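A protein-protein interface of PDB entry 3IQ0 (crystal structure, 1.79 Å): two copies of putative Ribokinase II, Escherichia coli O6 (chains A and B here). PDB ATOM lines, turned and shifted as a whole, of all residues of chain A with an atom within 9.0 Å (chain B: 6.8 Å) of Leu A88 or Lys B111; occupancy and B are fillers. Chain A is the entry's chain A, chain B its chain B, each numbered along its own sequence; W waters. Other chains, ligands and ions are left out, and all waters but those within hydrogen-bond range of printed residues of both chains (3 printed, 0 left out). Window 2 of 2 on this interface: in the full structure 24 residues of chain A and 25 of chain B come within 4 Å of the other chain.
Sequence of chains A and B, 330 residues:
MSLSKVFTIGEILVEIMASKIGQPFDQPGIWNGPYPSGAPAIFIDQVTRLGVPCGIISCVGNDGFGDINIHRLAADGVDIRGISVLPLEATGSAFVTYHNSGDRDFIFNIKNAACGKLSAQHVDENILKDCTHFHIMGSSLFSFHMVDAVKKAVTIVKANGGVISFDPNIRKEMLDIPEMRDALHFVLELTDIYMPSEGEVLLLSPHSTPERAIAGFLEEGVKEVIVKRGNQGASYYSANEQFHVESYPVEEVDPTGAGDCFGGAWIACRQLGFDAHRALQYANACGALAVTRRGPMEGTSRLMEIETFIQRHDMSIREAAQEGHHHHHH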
ATOM      1  N   VAL A  60      23.810 -12.372 -28.100  1.00  0.00           N
ATOM      2  CA  VAL A  60      23.182 -11.064 -27.955  1.00  0.00           C
ATOM      3  C   VAL A  60      22.358 -11.147 -26.689  1.00  0.00           C
ATOM      4  O   VAL A  60      22.149 -12.231 -26.148  1.00  0.00           O
ATOM      5  CB  VAL A  60      22.247 -10.706 -29.135  1.00  0.00           C
ATOM      6  CG1 VAL A  60      23.042 -10.648 -30.425  1.00  0.00           C
ATOM      7  CG2 VAL A  60      21.110 -11.712 -29.237  1.00  0.00           C
ATOM      8  N   GLY A  61      21.902 -10.004 -26.200  1.00  0.00           N
ATOM      9  CA  GLY A  61      21.099 -10.011 -24.998  1.00  0.00           C
ATOM     10  C   GLY A  61      19.647 -10.222 -25.359  1.00  0.00           C
ATOM     11  O   GLY A  61      19.279 -10.208 -26.530  1.00  0.00           O
ATOM     12  N   ASN A  62      18.817 -10.434 -24.352  1.00  0.00           N
ATOM     13  CA  ASN A  62      17.393 -10.627 -24.583  1.00  0.00           C
ATOM     14  C   ASN A  62      16.749  -9.241 -24.536  1.00  0.00           C
ATOM     15  O   ASN A  62      16.057  -8.895 -23.583  1.00  0.00           O
ATOM     16  CB  ASN A  62      16.826 -11.552 -23.502  1.00  0.00           C
ATOM     17  CG  ASN A  62      15.336 -11.728 -23.606  1.00  0.00           C
ATOM     18  OD1 ASN A  62      14.799 -11.990 -24.682  1.00  0.00           O
ATOM     19  ND2 ASN A  62      14.650 -11.598 -22.476  1.00  0.00           N
ATOM     20  N   ASP A  63      17.012  -8.448 -25.574  1.00  0.00           N
ATOM     21  CA  ASP A  63      16.484  -7.090 -25.683  1.00  0.00           C
ATOM     22  C   ASP A  63      16.300  -6.665 -27.144  1.00  0.00           C
ATOM     23  O   ASP A  63      16.689  -7.384 -28.068  1.00  0.00           O
ATOM     24  CB  ASP A  63      17.411  -6.094 -24.967  1.00  0.00           C
ATOM     25  CG  ASP A  63      18.854  -6.176 -25.443  1.00  0.00           C
ATOM     26  OD1 ASP A  63      19.090  -6.217 -26.665  1.00  0.00           O
ATOM     27  OD2 ASP A  63      19.762  -6.183 -24.590  1.00  0.00           O
ATOM     28  N   VAL A  85      20.895 -16.185 -27.110  1.00  0.00           N
ATOM     29  CA  VAL A  85      20.335 -15.023 -26.433  1.00  0.00           C
ATOM     30  C   VAL A  85      20.603 -15.166 -24.937  1.00  0.00           C
ATOM     31  O   VAL A  85      20.261 -16.180 -24.325  1.00  0.00           O
ATOM     32  CB  VAL A  85      18.825 -14.916 -26.696  1.00  0.00           C
ATOM     33  CG1 VAL A  85      18.244 -13.720 -25.961  1.00  0.00           C
ATOM     34  CG2 VAL A  85      18.583 -14.798 -28.194  1.00  0.00           C
ATOM     35  N   LEU A  86      21.234 -14.152 -24.361  1.00  0.00           N
ATOM     36  CA  LEU A  86      21.591 -14.163 -22.951  1.00  0.00           C
ATOM     37  C   LEU A  86      20.723 -13.211 -22.132  1.00  0.00           C
ATOM     38  O   LEU A  86      20.872 -11.992 -22.213  1.00  0.00           O
ATOM     39  CB  LEU A  86      23.070 -13.799 -22.800  1.00  0.00           C
ATOM     40  CG  LEU A  86      24.105 -14.876 -23.143  1.00  0.00           C
ATOM     41  CD1 LEU A  86      23.764 -15.561 -24.443  1.00  0.00           C
ATOM     42  CD2 LEU A  86      25.473 -14.245 -23.215  1.00  0.00           C
ATOM     43  N   PRO A  87      19.813 -13.770 -21.314  1.00  0.00           N
ATOM     44  CA  PRO A  87      18.863 -13.077 -20.434  1.00  0.00           C
ATOM     45  C   PRO A  87      19.463 -12.061 -19.466  1.00  0.00           C
ATOM     46  O   PRO A  87      18.862 -11.020 -19.206  1.00  0.00           O
ATOM     47  CB  PRO A  87      18.188 -14.224 -19.683  1.00  0.00           C
ATOM     48  CG  PRO A  87      18.276 -15.354 -20.632  1.00  0.00           C
ATOM     49  CD  PRO A  87      19.678 -15.229 -21.156  1.00  0.00           C
ATOM     50  N   LEU A  88      20.640 -12.362 -18.931  1.00  0.00           N
ATOM     51  CA  LEU A  88      21.278 -11.479 -17.962  1.00  0.00           C
ATOM     52  C   LEU A  88      22.311 -10.511 -18.541  1.00  0.00           C
ATOM     53  O   LEU A  88      22.955  -9.770 -17.796  1.00  0.00           O
ATOM     54  CB  LEU A  88      21.936 -12.323 -16.867  1.00  0.00           C
ATOM     55  CG  LEU A  88      21.031 -13.364 -16.200  1.00  0.00           C
ATOM     56  CD1 LEU A  88      21.849 -14.243 -15.264  1.00  0.00           C
ATOM     57  CD2 LEU A  88      19.906 -12.653 -15.453  1.00  0.00           C
ATOM     58  N   GLU A  89      22.467 -10.513 -19.860  1.00  0.00           N
ATOM     59  CA  GLU A  89      23.435  -9.638 -20.508  1.00  0.00           C
ATOM     60  C   GLU A  89      22.800  -8.675 -21.505  1.00  0.00           C
ATOM     61  O   GLU A  89      21.840  -9.020 -22.196  1.00  0.00           O
ATOM     62  CB  GLU A  89      24.488 -10.474 -21.243  1.00  0.00           C
ATOM     63  CG  GLU A  89      25.273 -11.437 -20.374  1.00  0.00           C
ATOM     64  CD  GLU A  89      26.173 -10.734 -19.379  1.00  0.00           C
ATOM     65  OE1 GLU A  89      26.958  -9.851 -19.798  1.00  0.00           O
ATOM     66  OE2 GLU A  89      26.097 -11.066 -18.178  1.00  0.00           O
ATOM     67  N   ALA A  90      23.354  -7.467 -21.585  1.00  0.00           N
ATOM     68  CA  ALA A  90      22.868  -6.464 -22.524  1.00  0.00           C
ATOM     69  C   ALA A  90      23.609  -6.650 -23.843  1.00  0.00           C
ATOM     70  O   ALA A  90      24.806  -6.926 -23.857  1.00  0.00           O
ATOM     71  CB  ALA A  90      23.122  -5.064 -21.982  1.00  0.00           C
ATOM     72  N   THR A  91      22.890  -6.511 -24.948  1.00  0.00           N
ATOM     73  CA  THR A  91      23.484  -6.632 -26.273  1.00  0.00           C
ATOM     74  C   THR A  91      24.542  -5.535 -26.404  1.00  0.00           C
ATOM     75  O   THR A  91      24.344  -4.418 -25.928  1.00  0.00           O
ATOM     76  CB  THR A  91      22.404  -6.455 -27.346  1.00  0.00           C
ATOM     77  OG1 THR A  91      21.446  -7.512 -27.215  1.00  0.00           O
ATOM     78  CG2 THR A  91      23.009  -6.466 -28.747  1.00  0.00           C
ATOM     79  N   ASN A 112      32.494  -6.289 -22.046  1.00  0.00           N
ATOM     80  CA  ASN A 112      31.637  -6.633 -20.918  1.00  0.00           C
ATOM     81  C   ASN A 112      30.152  -6.693 -21.245  1.00  0.00           C
ATOM     82  O   ASN A 112      29.312  -6.515 -20.365  1.00  0.00           O
ATOM     83  CB  ASN A 112      31.893  -5.650 -19.775  1.00  0.00           C
ATOM     84  CG  ASN A 112      33.345  -5.648 -19.341  1.00  0.00           C
ATOM     85  OD1 ASN A 112      33.979  -4.594 -19.237  1.00  0.00           O
ATOM     86  ND2 ASN A 112      33.883  -6.833 -19.091  1.00  0.00           N
ATOM     87  N   ALA A 113      29.843  -6.964 -22.511  1.00  0.00           N
ATOM     88  CA  ALA A 113      28.464  -7.071 -22.980  1.00  0.00           C
ATOM     89  C   ALA A 113      28.171  -8.513 -23.391  1.00  0.00           C
ATOM     90  O   ALA A 113      29.053  -9.367 -23.355  1.00  0.00           O
ATOM     91  CB  ALA A 113      28.237  -6.133 -24.167  1.00  0.00           C
ATOM     92  N   ALA A 114      26.932  -8.772 -23.792  1.00  0.00           N
ATOM     93  CA  ALA A 114      26.527 -10.117 -24.191  1.00  0.00           C
ATOM     94  C   ALA A 114      27.461 -10.745 -25.219  1.00  0.00           C
ATOM     95  O   ALA A 114      27.765 -11.929 -25.120  1.00  0.00           O
ATOM     96  CB  ALA A 114      25.099 -10.099 -24.733  1.00  0.00           C
ATOM     97  N   LYS A 117      30.382 -12.702 -23.983  1.00  0.00           N
ATOM     98  CA  LYS A 117      30.127 -13.917 -23.207  1.00  0.00           C
ATOM     99  C   LYS A 117      30.224 -15.163 -24.085  1.00  0.00           C
ATOM    100  O   LYS A 117      30.030 -16.289 -23.618  1.00  0.00           O
ATOM    101  CB  LYS A 117      28.743 -13.855 -22.553  1.00  0.00           C
ATOM    102  CG  LYS A 117      28.518 -12.632 -21.665  1.00  0.00           C
ATOM    103  CD  LYS A 117      29.553 -12.531 -20.547  1.00  0.00           C
ATOM    104  CE  LYS A 117      29.546 -13.768 -19.656  1.00  0.00           C
ATOM    105  NZ  LYS A 117      30.526 -13.684 -18.530  1.00  0.00           N
ATOM    106  N   PHE B 108      19.189  -1.529 -19.733  1.00  0.00           N
ATOM    107  CA  PHE B 108      20.240  -1.137 -18.797  1.00  0.00           C
ATOM    108  C   PHE B 108      21.591  -1.801 -18.978  1.00  0.00           C
ATOM    109  O   PHE B 108      21.687  -2.971 -19.351  1.00  0.00           O
ATOM    110  CB  PHE B 108      19.818  -1.438 -17.357  1.00  0.00           C
ATOM    111  CG  PHE B 108      18.680  -0.612 -16.862  1.00  0.00           C
ATOM    112  CD1 PHE B 108      18.824   0.761 -16.695  1.00  0.00           C
ATOM    113  CD2 PHE B 108      17.469  -1.209 -16.531  1.00  0.00           C
ATOM    114  CE1 PHE B 108      17.776   1.532 -16.201  1.00  0.00           C
ATOM    115  CE2 PHE B 108      16.413  -0.450 -16.037  1.00  0.00           C
ATOM    116  CZ  PHE B 108      16.565   0.921 -15.870  1.00  0.00           C
ATOM    117  N   ASN B 109      22.630  -1.029 -18.681  1.00  0.00           N
ATOM    118  CA  ASN B 109      24.002  -1.506 -18.678  1.00  0.00           C
ATOM    119  C   ASN B 109      24.627  -0.859 -17.453  1.00  0.00           C
ATOM    120  O   ASN B 109      25.331   0.140 -17.554  1.00  0.00           O
ATOM    121  CB  ASN B 109      24.791  -1.085 -19.906  1.00  0.00           C
ATOM    122  CG  ASN B 109      26.260  -1.464 -19.781  1.00  0.00           C
ATOM    123  OD1 ASN B 109      26.588  -2.569 -19.345  1.00  0.00           O
ATOM    124  ND2 ASN B 109      27.145  -0.553 -20.150  1.00  0.00           N
ATOM    125  N   ILE B 110      24.345  -1.433 -16.292  1.00  0.00           N
ATOM    126  CA  ILE B 110      24.858  -0.908 -15.039  1.00  0.00           C
ATOM    127  C   ILE B 110      25.653  -1.971 -14.288  1.00  0.00           C
ATOM    128  O   ILE B 110      26.812  -1.769 -13.940  1.00  0.00           O
ATOM    129  CB  ILE B 110      23.695  -0.443 -14.143  1.00  0.00           C
ATOM    130  CG1 ILE B 110      22.920   0.679 -14.837  1.00  0.00           C
ATOM    131  CG2 ILE B 110      24.223  -0.021 -12.779  1.00  0.00           C
ATOM    132  CD1 ILE B 110      21.638   1.062 -14.118  1.00  0.00           C
ATOM    133  N   LYS B 111      25.001  -3.100 -14.038  1.00  0.00           N
ATOM    134  CA  LYS B 111      25.598  -4.218 -13.316  1.00  0.00           C
ATOM    135  C   LYS B 111      26.951  -4.628 -13.884  1.00  0.00           C
ATOM    136  O   LYS B 111      27.878  -4.943 -13.135  1.00  0.00           O
ATOM    137  CB  LYS B 111      24.646  -5.414 -13.357  1.00  0.00           C
ATOM    138  CG  LYS B 111      25.113  -6.628 -12.566  1.00  0.00           C
ATOM    139  CD  LYS B 111      24.947  -7.904 -13.384  1.00  0.00           C
ATOM    140  CE  LYS B 111      23.532  -8.039 -13.936  1.00  0.00           C
ATOM    141  NZ  LYS B 111      23.426  -9.136 -14.945  1.00  0.00           N
ATOM    142  N   ASN B 112      27.061  -4.622 -15.209  1.00  0.00           N
ATOM    143  CA  ASN B 112      28.297  -5.012 -15.870  1.00  0.00           C
ATOM    144  C   ASN B 112      29.118  -3.859 -16.424  1.00  0.00           C
ATOM    145  O   ASN B 112      29.974  -4.066 -17.280  1.00  0.00           O
ATOM    146  CB  ASN B 112      27.993  -6.001 -16.996  1.00  0.00           C
ATOM    147  CG  ASN B 112      27.434  -7.299 -16.480  1.00  0.00           C
ATOM    148  OD1 ASN B 112      28.046  -7.949 -15.634  1.00  0.00           O
ATOM    149  ND2 ASN B 112      26.264  -7.687 -16.978  1.00  0.00           N
ATOM    150  N   ALA B 113      28.860  -2.651 -15.939  1.00  0.00           N
ATOM    151  CA  ALA B 113      29.598  -1.479 -16.391  1.00  0.00           C
ATOM    152  C   ALA B 113      30.449  -0.926 -15.249  1.00  0.00           C
ATOM    153  O   ALA B 113      30.634  -1.584 -14.225  1.00  0.00           O
ATOM    154  CB  ALA B 113      28.627  -0.408 -16.888  1.00  0.00           C
ATOM    155  N   ALA B 114      30.967   0.283 -15.426  1.00  0.00           N
ATOM    156  CA  ALA B 114      31.787   0.915 -14.402  1.00  0.00           C
ATOM    157  C   ALA B 114      31.076   0.900 -13.050  1.00  0.00           C
ATOM    158  O   ALA B 114      31.694   0.637 -12.016  1.00  0.00           O
ATOM    159  CB  ALA B 114      32.110   2.345 -14.806  1.00  0.00           C
ATOM    160  N   CYS B 115      29.772   1.164 -13.068  1.00  0.00           N
ATOM    161  CA  CYS B 115      28.968   1.200 -11.849  1.00  0.00           C
ATOM    162  C   CYS B 115      29.250   0.030 -10.915  1.00  0.00           C
ATOM    163  O   CYS B 115      29.633   0.222  -9.761  1.00  0.00           O
ATOM    164  CB  CYS B 115      27.476   1.190 -12.192  1.00  0.00           C
ATOM    165  SG  CYS B 115      27.001   2.241 -13.564  1.00  0.00           S
ATOM    166  N   GLY B 116      29.046  -1.184 -11.417  1.00  0.00           N
ATOM    167  CA  GLY B 116      29.260  -2.371 -10.611  1.00  0.00           C
ATOM    168  C   GLY B 116      30.702  -2.678 -10.264  1.00  0.00           C
ATOM    169  O   GLY B 116      30.997  -3.774  -9.791  1.00  0.00           O
ATOM    170  N   LYS B 117      31.594  -1.717 -10.490  1.00  0.00           N
ATOM    171  CA  LYS B 117      33.015  -1.890 -10.187  1.00  0.00           C
ATOM    172  C   LYS B 117      33.391  -1.195  -8.878  1.00  0.00           C
ATOM    173  O   LYS B 117      34.499  -1.359  -8.371  1.00  0.00           O
ATOM    174  CB  LYS B 117      33.869  -1.315 -11.312  1.00  0.00           C
ATOM    175  CG  LYS B 117      34.973  -2.237 -11.799  1.00  0.00           C
ATOM    176  CD  LYS B 117      34.526  -3.074 -12.990  1.00  0.00           C
ATOM    177  CE  LYS B 117      33.509  -4.131 -12.610  1.00  0.00           C
ATOM    178  NZ  LYS B 117      34.126  -5.229 -11.835  1.00  0.00           N
ATOM    179  N   PHE B 142      23.448  -4.167  -5.796  1.00  0.00           N
ATOM    180  CA  PHE B 142      23.187  -5.249  -6.736  1.00  0.00           C
ATOM    181  C   PHE B 142      24.350  -6.232  -6.862  1.00  0.00           C
ATOM    182  O   PHE B 142      24.387  -7.042  -7.789  1.00  0.00           O
ATOM    183  CB  PHE B 142      22.819  -4.678  -8.117  1.00  0.00           C
ATOM    184  CG  PHE B 142      23.846  -3.729  -8.695  1.00  0.00           C
ATOM    185  CD1 PHE B 142      25.071  -4.196  -9.157  1.00  0.00           C
ATOM    186  CD2 PHE B 142      23.568  -2.367  -8.802  1.00  0.00           C
ATOM    187  CE1 PHE B 142      26.007  -3.322  -9.720  1.00  0.00           C
ATOM    188  CE2 PHE B 142      24.495  -1.487  -9.361  1.00  0.00           C
ATOM    189  CZ  PHE B 142      25.715  -1.964  -9.822  1.00  0.00           C
ATOM    190  N   SER B 143      25.292  -6.161  -5.925  1.00  0.00           N
ATOM    191  CA  SER B 143      26.451  -7.056  -5.914  1.00  0.00           C
ATOM    192  C   SER B 143      27.129  -6.981  -4.549  1.00  0.00           C
ATOM    193  O   SER B 143      26.986  -5.985  -3.837  1.00  0.00           O
ATOM    194  CB  SER B 143      27.456  -6.669  -7.004  1.00  0.00           C
ATOM    195  OG  SER B 143      28.364  -5.688  -6.542  1.00  0.00           O
ATOM    196  N   ARG B 171      14.909  -3.189  -6.869  1.00  0.00           N
ATOM    197  CA  ARG B 171      14.188  -3.971  -7.862  1.00  0.00           C
ATOM    198  C   ARG B 171      13.711  -5.154  -7.028  1.00  0.00           C
ATOM    199  O   ARG B 171      14.529  -5.907  -6.491  1.00  0.00           O
ATOM    200  CB  ARG B 171      15.132  -4.470  -8.955  1.00  0.00           C
ATOM    201  CG  ARG B 171      15.790  -3.380  -9.773  1.00  0.00           C
ATOM    202  CD  ARG B 171      16.838  -3.974 -10.699  1.00  0.00           C
ATOM    203  NE  ARG B 171      16.251  -4.829 -11.727  1.00  0.00           N
ATOM    204  CZ  ARG B 171      16.827  -5.932 -12.197  1.00  0.00           C
ATOM    205  NH1 ARG B 171      18.007  -6.317 -11.727  1.00  0.00           N
ATOM    206  NH2 ARG B 171      16.224  -6.654 -13.131  1.00  0.00           N
HETATM  207  O   HOH W   1      25.979  -7.029 -19.851  1.00  0.00           O
HETATM  208  O   HOH W   2      25.330 -11.050 -15.582  1.00  0.00           O
HETATM  209  O   HOH W   3      27.134  -4.756 -20.483  1.00  0.00           O
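The backbone carbonyl oxygen (O) of Leu A88 sits at hydrogen-bond distance from the side-chain amino group (NZ) of Lys B111, at 3.0 Å.
The backbone carbonyl oxygen (O) of Ala A90 lies within hydrogen-bond range of the backbone NH (N) of Ala A114, at 2.8 Å.
Among the printed residues, merely in contact across the chains: Leu A88 with Asn B112 (3.99 Å), Glu A89 with Asn B112 (3.6 Å), Ala A90 with Phe B108 (3.7 Å) and Asn A112 with Asn B112 (3.5 Å).
Of the printed residues of chain B, Leu A88 touches Lys B111 (3.0 Å) and Asn B112 (3.99 Å).
Of chain A, only Leu A88 (3.0 Å) comes within 4 Å of Lys B111.
No residue of chain A comes within 4 Å of Gly B116.
Of the printed residues of chain A, Phe B108 touches Ala A90 (3.7 Å).
Of the printed residues of chain B, Ala A90 touches Phe B108.
Printed residues of chain B within 4 Å of Asn A112: Asn B112.
Of the printed residues of chain A, Asn B112 touches Leu A88 (3.99 Å), Glu A89 (3.6 Å) and Asn A112 (3.5 Å).
Printed residues of chain B within 4 Å of Glu A89: Asn B112 (3.6 Å).
Thr A91 touches none of the printed residues of chain B.
Ala B114 touches none of the printed residues of chain A.
The nearest printed residue of chain B that does not touch Leu A88 is Phe B108 (7.1 Å).
The nearest residue of chain A that does not touch Lys B111 is Glu A89 (4.6 Å).
Printed residues of chain A that touch a printed residue of chain B: Leu A88, Glu A89, Ala A90 and Asn A112.
Hydrophobic or aromatic side chains of chain A within 4 Å of the printed part of chain B: Ala A90.
Among the printed residues, 5 pairs touch across the chains.
Among the printed residues, no Asp or Glu carboxylate lies within 4 Å of a Lys or Arg side-chain nitrogen of the other chain.
Asn B112 touches its own counterpart, Asn A112.
Of the 5 pairs that touch across the chains among the printed residues, 1 has its exchanged pair printed and touching as well.
Water W3 lies within hydrogen-bond range of OD1 of Asn B109 and O of Asn A112.
Water W2 lies within hydrogen-bond range of the side-chain carboxylate of Glu A89 (2.7 Å), the side-chain amino group of Lys B111 (2.8 Å) and the backbone carbonyl oxygen of Leu A88 (3.5 Å).
Water W1 lies within hydrogen-bond range of ND2 of Asn B112 (3.0 Å), OE1 of Glu A89 (3.0 Å), N of Ala A90 (3.2 Å) and O of Asn A112 (3.4 Å).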
